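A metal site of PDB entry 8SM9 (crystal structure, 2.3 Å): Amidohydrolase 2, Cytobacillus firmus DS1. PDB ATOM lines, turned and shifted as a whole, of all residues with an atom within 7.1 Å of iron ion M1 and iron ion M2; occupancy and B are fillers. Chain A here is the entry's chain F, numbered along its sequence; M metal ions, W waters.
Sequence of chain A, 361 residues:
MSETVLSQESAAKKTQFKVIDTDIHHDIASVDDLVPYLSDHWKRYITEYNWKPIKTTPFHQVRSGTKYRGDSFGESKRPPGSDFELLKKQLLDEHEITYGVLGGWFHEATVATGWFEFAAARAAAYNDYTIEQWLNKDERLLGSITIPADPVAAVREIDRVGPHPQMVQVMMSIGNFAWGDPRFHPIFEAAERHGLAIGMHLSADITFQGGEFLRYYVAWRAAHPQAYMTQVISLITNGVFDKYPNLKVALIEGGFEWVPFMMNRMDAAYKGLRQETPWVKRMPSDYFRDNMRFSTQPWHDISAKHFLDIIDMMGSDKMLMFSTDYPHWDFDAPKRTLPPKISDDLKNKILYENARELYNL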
ATOM      1  N   ASP A  23       0.382   7.487  12.241  1.00  0.00           N
ATOM      2  CA  ASP A  23       0.351   6.027  12.319  1.00  0.00           C
ATOM      3  C   ASP A  23       0.413   5.573  13.775  1.00  0.00           C
ATOM      4  O   ASP A  23       1.498   5.438  14.346  1.00  0.00           O
ATOM      5  CB  ASP A  23       1.492   5.406  11.521  1.00  0.00           C
ATOM      6  CG  ASP A  23       1.263   3.933  11.245  1.00  0.00           C
ATOM      7  OD1 ASP A  23       0.120   3.451  11.462  1.00  0.00           O
ATOM      8  OD2 ASP A  23       2.218   3.257  10.805  1.00  0.00           O
ATOM      9  N   ILE A  24      -0.753   5.309  14.357  1.00  0.00           N
ATOM     10  CA  ILE A  24      -0.875   4.763  15.699  1.00  0.00           C
ATOM     11  C   ILE A  24      -1.720   3.502  15.614  1.00  0.00           C
ATOM     12  O   ILE A  24      -2.762   3.497  14.940  1.00  0.00           O
ATOM     13  CB  ILE A  24      -1.527   5.780  16.659  1.00  0.00           C
ATOM     14  CG1 ILE A  24      -0.715   7.061  16.649  1.00  0.00           C
ATOM     15  CG2 ILE A  24      -1.673   5.182  18.045  1.00  0.00           C
ATOM     16  CD1 ILE A  24      -1.416   8.224  17.310  1.00  0.00           C
ATOM     17  N   HIS A  25      -1.302   2.449  16.314  1.00  0.00           N
ATOM     18  CA  HIS A  25      -1.913   1.122  16.149  1.00  0.00           C
ATOM     19  C   HIS A  25      -2.628   0.680  17.413  1.00  0.00           C
ATOM     20  O   HIS A  25      -2.189  -0.247  18.105  1.00  0.00           O
ATOM     21  CB  HIS A  25      -0.859   0.115  15.750  1.00  0.00           C
ATOM     22  CG  HIS A  25      -0.382   0.295  14.356  1.00  0.00           C
ATOM     23  ND1 HIS A  25      -1.224   0.238  13.271  1.00  0.00           N
ATOM     24  CD2 HIS A  25       0.855   0.557  13.863  1.00  0.00           C
ATOM     25  CE1 HIS A  25      -0.529   0.431  12.165  1.00  0.00           C
ATOM     26  NE2 HIS A  25       0.730   0.626  12.501  1.00  0.00           N
ATOM     27  N   GLN A  61      10.019 -10.482  14.105  1.00  0.00           N
ATOM     28  CA  GLN A  61      11.236  -9.941  14.708  1.00  0.00           C
ATOM     29  C   GLN A  61      11.825 -10.914  15.734  1.00  0.00           C
ATOM     30  O   GLN A  61      11.195 -11.199  16.760  1.00  0.00           O
ATOM     31  CB  GLN A  61      10.959  -8.610  15.388  1.00  0.00           C
ATOM     32  CG  GLN A  61      10.449  -7.533  14.493  1.00  0.00           C
ATOM     33  CD  GLN A  61       8.988  -7.716  14.194  1.00  0.00           C
ATOM     34  OE1 GLN A  61       8.347  -8.650  14.699  1.00  0.00           O
ATOM     35  NE2 GLN A  61       8.439  -6.830  13.356  1.00  0.00           N
ATOM     36  N   LYS A  67       7.428  -7.253  17.688  1.00  0.00           N
ATOM     37  CA  LYS A  67       7.207  -6.015  16.922  1.00  0.00           C
ATOM     38  C   LYS A  67       6.810  -4.853  17.833  1.00  0.00           C
ATOM     39  O   LYS A  67       6.368  -3.836  17.299  1.00  0.00           O
ATOM     40  CB  LYS A  67       6.052  -6.292  15.960  1.00  0.00           C
ATOM     41  CG  LYS A  67       5.251  -7.547  16.262  1.00  0.00           C
ATOM     42  CD  LYS A  67       3.779  -7.293  16.452  1.00  0.00           C
ATOM     43  CE  LYS A  67       3.052  -6.949  15.168  1.00  0.00           C
ATOM     44  NZ  LYS A  67       2.412  -5.627  15.243  1.00  0.00           N
ATOM     45  N   GLY A 104      -5.263   1.348  13.700  1.00  0.00           N
ATOM     46  CA  GLY A 104      -5.703   0.052  14.129  1.00  0.00           C
ATOM     47  C   GLY A 104      -4.752  -1.066  13.754  1.00  0.00           C
ATOM     48  O   GLY A 104      -3.707  -0.827  13.140  1.00  0.00           O
ATOM     49  N   TRP A 105      -5.124  -2.274  14.126  1.00  0.00           N
ATOM     50  CA  TRP A 105      -4.418  -3.473  13.718  1.00  0.00           C
ATOM     51  C   TRP A 105      -5.405  -4.466  13.152  1.00  0.00           C
ATOM     52  O   TRP A 105      -5.444  -5.627  13.528  1.00  0.00           O
ATOM     53  CB  TRP A 105      -3.638  -4.091  14.889  1.00  0.00           C
ATOM     54  CG  TRP A 105      -2.485  -4.925  14.419  1.00  0.00           C
ATOM     55  CD1 TRP A 105      -2.267  -6.244  14.709  1.00  0.00           C
ATOM     56  CD2 TRP A 105      -1.412  -4.515  13.549  1.00  0.00           C
ATOM     57  NE1 TRP A 105      -1.109  -6.674  14.081  1.00  0.00           N
ATOM     58  CE2 TRP A 105      -0.575  -5.635  13.369  1.00  0.00           C
ATOM     59  CE3 TRP A 105      -1.069  -3.311  12.919  1.00  0.00           C
ATOM     60  CZ2 TRP A 105       0.580  -5.588  12.586  1.00  0.00           C
ATOM     61  CZ3 TRP A 105       0.076  -3.265  12.125  1.00  0.00           C
ATOM     62  CH2 TRP A 105       0.894  -4.400  11.974  1.00  0.00           C
ATOM     63  N   HIS A 107      -6.099  -5.030   9.679  1.00  0.00           N
ATOM     64  CA  HIS A 107      -5.964  -5.324   8.264  1.00  0.00           C
ATOM     65  C   HIS A 107      -6.426  -6.739   7.887  1.00  0.00           C
ATOM     66  O   HIS A 107      -6.654  -7.007   6.698  1.00  0.00           O
ATOM     67  CB  HIS A 107      -4.514  -5.126   7.842  1.00  0.00           C
ATOM     68  CG  HIS A 107      -3.984  -3.790   8.230  1.00  0.00           C
ATOM     69  ND1 HIS A 107      -4.506  -2.607   7.746  1.00  0.00           N
ATOM     70  CD2 HIS A 107      -3.005  -3.440   9.096  1.00  0.00           C
ATOM     71  CE1 HIS A 107      -3.860  -1.599   8.282  1.00  0.00           C
ATOM     72  NE2 HIS A 107      -2.941  -2.069   9.110  1.00  0.00           N
ATOM     73  N   HIS A 201      -1.593   1.089   4.346  1.00  0.00           N
ATOM     74  CA  HIS A 201      -0.641   0.546   5.302  1.00  0.00           C
ATOM     75  C   HIS A 201      -0.390  -0.930   4.997  1.00  0.00           C
ATOM     76  O   HIS A 201      -1.321  -1.659   4.647  1.00  0.00           O
ATOM     77  CB  HIS A 201      -1.217   0.716   6.702  1.00  0.00           C
ATOM     78  CG  HIS A 201      -0.231   0.502   7.793  1.00  0.00           C
ATOM     79  ND1 HIS A 201       0.139  -0.747   8.228  1.00  0.00           N
ATOM     80  CD2 HIS A 201       0.458   1.381   8.556  1.00  0.00           C
ATOM     81  CE1 HIS A 201       1.025  -0.636   9.204  1.00  0.00           C
ATOM     82  NE2 HIS A 201       1.220   0.646   9.429  1.00  0.00           N
ATOM     83  N   LEU A 202       0.854  -1.380   5.147  1.00  0.00           N
ATOM     84  CA  LEU A 202       1.153  -2.789   4.880  1.00  0.00           C
ATOM     85  C   LEU A 202       0.287  -3.702   5.754  1.00  0.00           C
ATOM     86  O   LEU A 202      -0.181  -3.309   6.823  1.00  0.00           O
ATOM     87  CB  LEU A 202       2.623  -3.085   5.140  1.00  0.00           C
ATOM     88  CG  LEU A 202       3.102  -2.422   6.437  1.00  0.00           C
ATOM     89  CD1 LEU A 202       2.819  -3.230   7.714  1.00  0.00           C
ATOM     90  CD2 LEU A 202       4.573  -2.108   6.367  1.00  0.00           C
ATOM     91  N   TYR A 217      12.367 -12.742   8.005  1.00  0.00           N
ATOM     92  CA  TYR A 217      11.655 -11.485   8.215  1.00  0.00           C
ATOM     93  C   TYR A 217      12.538 -10.293   7.863  1.00  0.00           C
ATOM     94  O   TYR A 217      12.029  -9.261   7.388  1.00  0.00           O
ATOM     95  CB  TYR A 217      11.159 -11.373   9.661  1.00  0.00           C
ATOM     96  CG  TYR A 217      10.726  -9.952   9.998  1.00  0.00           C
ATOM     97  CD1 TYR A 217       9.493  -9.456   9.580  1.00  0.00           C
ATOM     98  CD2 TYR A 217      11.551  -9.101  10.709  1.00  0.00           C
ATOM     99  CE1 TYR A 217       9.106  -8.140   9.875  1.00  0.00           C
ATOM    100  CE2 TYR A 217      11.171  -7.800  11.000  1.00  0.00           C
ATOM    101  CZ  TYR A 217       9.959  -7.331  10.593  1.00  0.00           C
ATOM    102  OH  TYR A 217       9.597  -6.033  10.896  1.00  0.00           O
ATOM    103  N   ARG A 221      10.997  -7.470   5.597  1.00  0.00           N
ATOM    104  CA  ARG A 221      11.048  -6.052   5.960  1.00  0.00           C
ATOM    105  C   ARG A 221      11.675  -5.226   4.850  1.00  0.00           C
ATOM    106  O   ARG A 221      11.124  -4.196   4.440  1.00  0.00           O
ATOM    107  CB  ARG A 221      11.842  -5.888   7.260  1.00  0.00           C
ATOM    108  CG  ARG A 221      11.621  -4.593   7.987  1.00  0.00           C
ATOM    109  CD  ARG A 221      12.601  -4.411   9.140  1.00  0.00           C
ATOM    110  NE  ARG A 221      12.593  -3.014   9.566  1.00  0.00           N
ATOM    111  CZ  ARG A 221      11.596  -2.436  10.230  1.00  0.00           C
ATOM    112  NH1 ARG A 221      10.536  -3.128  10.654  1.00  0.00           N
ATOM    113  NH2 ARG A 221      11.658  -1.128  10.477  1.00  0.00           N
ATOM    114  N   TYR A 228       4.135  -0.845  -1.712  1.00  0.00           N
ATOM    115  CA  TYR A 228       3.741   0.559  -1.767  1.00  0.00           C
ATOM    116  C   TYR A 228       3.959   1.116  -3.158  1.00  0.00           C
ATOM    117  O   TYR A 228       3.149   1.893  -3.669  1.00  0.00           O
ATOM    118  CB  TYR A 228       4.530   1.368  -0.747  1.00  0.00           C
ATOM    119  CG  TYR A 228       4.109   1.148   0.686  1.00  0.00           C
ATOM    120  CD1 TYR A 228       4.462  -0.015   1.367  1.00  0.00           C
ATOM    121  CD2 TYR A 228       3.364   2.117   1.363  1.00  0.00           C
ATOM    122  CE1 TYR A 228       4.092  -0.222   2.687  1.00  0.00           C
ATOM    123  CE2 TYR A 228       2.976   1.920   2.689  1.00  0.00           C
ATOM    124  CZ  TYR A 228       3.354   0.757   3.337  1.00  0.00           C
ATOM    125  OH  TYR A 228       2.995   0.572   4.637  1.00  0.00           O
ATOM    126  N   ILE A 252       1.678   5.098   4.273  1.00  0.00           N
ATOM    127  CA  ILE A 252       2.070   5.145   5.664  1.00  0.00           C
ATOM    128  C   ILE A 252       2.943   3.926   5.915  1.00  0.00           C
ATOM    129  O   ILE A 252       2.441   2.800   5.894  1.00  0.00           O
ATOM    130  CB  ILE A 252       0.839   5.143   6.569  1.00  0.00           C
ATOM    131  CG1 ILE A 252       0.008   6.395   6.325  1.00  0.00           C
ATOM    132  CG2 ILE A 252       1.235   5.028   8.016  1.00  0.00           C
ATOM    133  CD1 ILE A 252      -1.265   6.397   7.087  1.00  0.00           C
ATOM    134  N   GLU A 253       4.244   4.167   6.124  1.00  0.00           N
ATOM    135  CA  GLU A 253       5.226   3.176   6.585  1.00  0.00           C
ATOM    136  C   GLU A 253       5.818   2.406   5.414  1.00  0.00           C
ATOM    137  O   GLU A 253       6.393   1.319   5.598  1.00  0.00           O
ATOM    138  CB  GLU A 253       4.625   2.211   7.634  1.00  0.00           C
ATOM    139  CG  GLU A 253       5.690   1.612   8.560  1.00  0.00           C
ATOM    140  CD  GLU A 253       5.145   0.846   9.754  1.00  0.00           C
ATOM    141  OE1 GLU A 253       4.009   1.087  10.168  1.00  0.00           O
ATOM    142  OE2 GLU A 253       5.871  -0.016  10.290  1.00  0.00           O
ATOM    143  N   GLN A 297       8.152   7.497   9.078  1.00  0.00           N
ATOM    144  CA  GLN A 297       8.465   6.282   9.845  1.00  0.00           C
ATOM    145  C   GLN A 297       8.516   5.060   8.913  1.00  0.00           C
ATOM    146  O   GLN A 297       7.618   4.875   8.077  1.00  0.00           O
ATOM    147  CB  GLN A 297       7.405   6.073  10.935  1.00  0.00           C
ATOM    148  CG  GLN A 297       7.779   5.134  12.064  1.00  0.00           C
ATOM    149  CD  GLN A 297       7.643   3.692  11.646  1.00  0.00           C
ATOM    150  OE1 GLN A 297       6.938   3.395  10.694  1.00  0.00           O
ATOM    151  NE2 GLN A 297       8.336   2.797  12.347  1.00  0.00           N
ATOM    152  N   SER A 323       5.020  10.176  11.609  1.00  0.00           N
ATOM    153  CA  SER A 323       4.283   9.266  12.472  1.00  0.00           C
ATOM    154  C   SER A 323       5.248   8.605  13.434  1.00  0.00           C
ATOM    155  O   SER A 323       6.455   8.515  13.174  1.00  0.00           O
ATOM    156  CB  SER A 323       3.519   8.206  11.675  1.00  0.00           C
ATOM    157  OG  SER A 323       4.402   7.475  10.868  1.00  0.00           O
ATOM    158  N   THR A 324       4.716   8.142  14.567  1.00  0.00           N
ATOM    159  CA  THR A 324       5.528   7.442  15.545  1.00  0.00           C
ATOM    160  C   THR A 324       5.534   5.944  15.345  1.00  0.00           C
ATOM    161  O   THR A 324       6.526   5.299  15.705  1.00  0.00           O
ATOM    162  CB  THR A 324       5.029   7.695  16.965  1.00  0.00           C
ATOM    163  OG1 THR A 324       3.715   7.139  17.093  1.00  0.00           O
ATOM    164  CG2 THR A 324       5.055   9.167  17.326  1.00  0.00           C
ATOM    165  N   ASP A 325       4.444   5.391  14.801  1.00  0.00           N
ATOM    166  CA  ASP A 325       4.222   3.959  14.715  1.00  0.00           C
ATOM    167  C   ASP A 325       4.057   3.329  16.092  1.00  0.00           C
ATOM    168  O   ASP A 325       4.377   2.148  16.282  1.00  0.00           O
ATOM    169  CB  ASP A 325       5.342   3.249  13.932  1.00  0.00           C
ATOM    170  CG  ASP A 325       4.882   1.939  13.338  1.00  0.00           C
ATOM    171  OD1 ASP A 325       3.659   1.742  13.198  1.00  0.00           O
ATOM    172  OD2 ASP A 325       5.735   1.096  13.011  1.00  0.00           O
ATOM    173  N   TYR A 326       3.565   4.089  17.051  1.00  0.00           N
ATOM    174  CA  TYR A 326       3.253   3.532  18.355  1.00  0.00           C
ATOM    175  C   TYR A 326       2.225   2.424  18.194  1.00  0.00           C
ATOM    176  O   TYR A 326       1.198   2.630  17.518  1.00  0.00           O
ATOM    177  CB  TYR A 326       2.726   4.629  19.293  1.00  0.00           C
ATOM    178  CG  TYR A 326       2.388   4.131  20.690  1.00  0.00           C
ATOM    179  CD1 TYR A 326       1.148   3.542  20.973  1.00  0.00           C
ATOM    180  CD2 TYR A 326       3.318   4.241  21.732  1.00  0.00           C
ATOM    181  CE1 TYR A 326       0.848   3.077  22.259  1.00  0.00           C
ATOM    182  CE2 TYR A 326       3.020   3.784  23.015  1.00  0.00           C
ATOM    183  CZ  TYR A 326       1.787   3.205  23.272  1.00  0.00           C
ATOM    184  OH  TYR A 326       1.493   2.749  24.533  1.00  0.00           O
ATOM    185  N   HIS A 328       4.977   0.159  17.969  1.00  0.00           N
ATOM    186  CA  HIS A 328       5.853  -0.848  17.407  1.00  0.00           C
ATOM    187  C   HIS A 328       7.303  -0.616  17.815  1.00  0.00           C
ATOM    188  O   HIS A 328       7.682   0.444  18.339  1.00  0.00           O
ATOM    189  CB  HIS A 328       5.679  -0.924  15.899  1.00  0.00           C
ATOM    190  CG  HIS A 328       4.380  -1.533  15.497  1.00  0.00           C
ATOM    191  ND1 HIS A 328       3.994  -1.688  14.184  1.00  0.00           N
ATOM    192  CD2 HIS A 328       3.367  -2.036  16.254  1.00  0.00           C
ATOM    193  CE1 HIS A 328       2.796  -2.251  14.153  1.00  0.00           C
ATOM    194  NE2 HIS A 328       2.402  -2.471  15.391  1.00  0.00           N
ATOM    195  N   TRP A 329       8.131  -1.632  17.571  1.00  0.00           N
ATOM    196  CA  TRP A 329       9.481  -1.654  18.106  1.00  0.00           C
ATOM    197  C   TRP A 329      10.366  -0.570  17.496  1.00  0.00           C
ATOM    198  O   TRP A 329      11.331  -0.133  18.142  1.00  0.00           O
ATOM    199  CB  TRP A 329      10.084  -3.059  17.881  1.00  0.00           C
ATOM    200  CG  TRP A 329      10.348  -3.402  16.411  1.00  0.00           C
ATOM    201  CD1 TRP A 329       9.414  -3.745  15.467  1.00  0.00           C
ATOM    202  CD2 TRP A 329      11.621  -3.431  15.747  1.00  0.00           C
ATOM    203  NE1 TRP A 329      10.032  -3.969  14.252  1.00  0.00           N
ATOM    204  CE2 TRP A 329      11.387  -3.790  14.389  1.00  0.00           C
ATOM    205  CE3 TRP A 329      12.945  -3.197  16.154  1.00  0.00           C
ATOM    206  CZ2 TRP A 329      12.424  -3.912  13.449  1.00  0.00           C
ATOM    207  CZ3 TRP A 329      13.979  -3.299  15.205  1.00  0.00           C
ATOM    208  CH2 TRP A 329      13.710  -3.658  13.869  1.00  0.00           C
ATOM    209  N   ASP A 330      10.071  -0.113  16.275  1.00  0.00           N
ATOM    210  CA  ASP A 330      10.821   0.961  15.625  1.00  0.00           C
ATOM    211  C   ASP A 330      10.079   2.297  15.694  1.00  0.00           C
ATOM    212  O   ASP A 330      10.056   3.090  14.757  1.00  0.00           O
ATOM    213  CB  ASP A 330      11.170   0.598  14.186  1.00  0.00           C
ATOM    214  CG  ASP A 330       9.964   0.159  13.367  1.00  0.00           C
ATOM    215  OD1 ASP A 330       8.886  -0.158  13.959  1.00  0.00           O
ATOM    216  OD2 ASP A 330      10.110   0.137  12.120  1.00  0.00           O
HETATM  217 FE    FE M   1       2.524   1.081  11.355  1.00  0.00          FE
HETATM  218 FE    FE M   2       5.140  -0.900  12.160  1.00  0.00          FE
HETATM  219  O   HOH W   1       3.412  -1.622  11.532  1.00  0.00           O
HETATM  220  O   HOH W   2       7.017  -1.637  12.649  1.00  0.00           O
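Of the 23 residues printed, 3 come within 4 Å of iron ion M2.
Water W1 is bound to iron ion M2, at 2.0 Å.
Iron ion M2 is bound by water W2, at 2.1 Å.
Iron ion M2 is bound by OE2 of Glu 253 (2.2 Å).
Iron ion M2 is bound by the side-chain carboxylate (OD2) of Asp 325 (2.2 Å).
Iron ion M2 is bound by a ring nitrogen (ND1) of His 328 (2.5 Å).
The backbone NH (N) of His 25 lies within hydrogen-bond range of the backbone carbonyl oxygen (O) of Tyr 326, 2.8 Å away.
ND1 of His 25 is in hydrogen-bond range of O of Gly 104 (2.7 Å).
NE2 of Gln 297 sits close to OD2 of Asp 325 (3.2 Å).
A ring nitrogen (NE2) of His 107 is in hydrogen-bond range of a ring nitrogen (ND1) of His 201, 3.5 Å away.
The side-chain amino group (NZ) of Lys 67 lies within hydrogen-bond range of a ring nitrogen (NE2) of His 328.
Of the 23 residues printed, 5 come within 4 Å of iron ion M1.
Iron ion M1 is bound by OE1 of Glu 253 (1.9 Å), NE2 of His 25 (2.2 Å), OD1 of Asp 325 (2.3 Å), OD2 of Asp 23 (2.3 Å) and NE2 of His 201 (2.4 Å).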
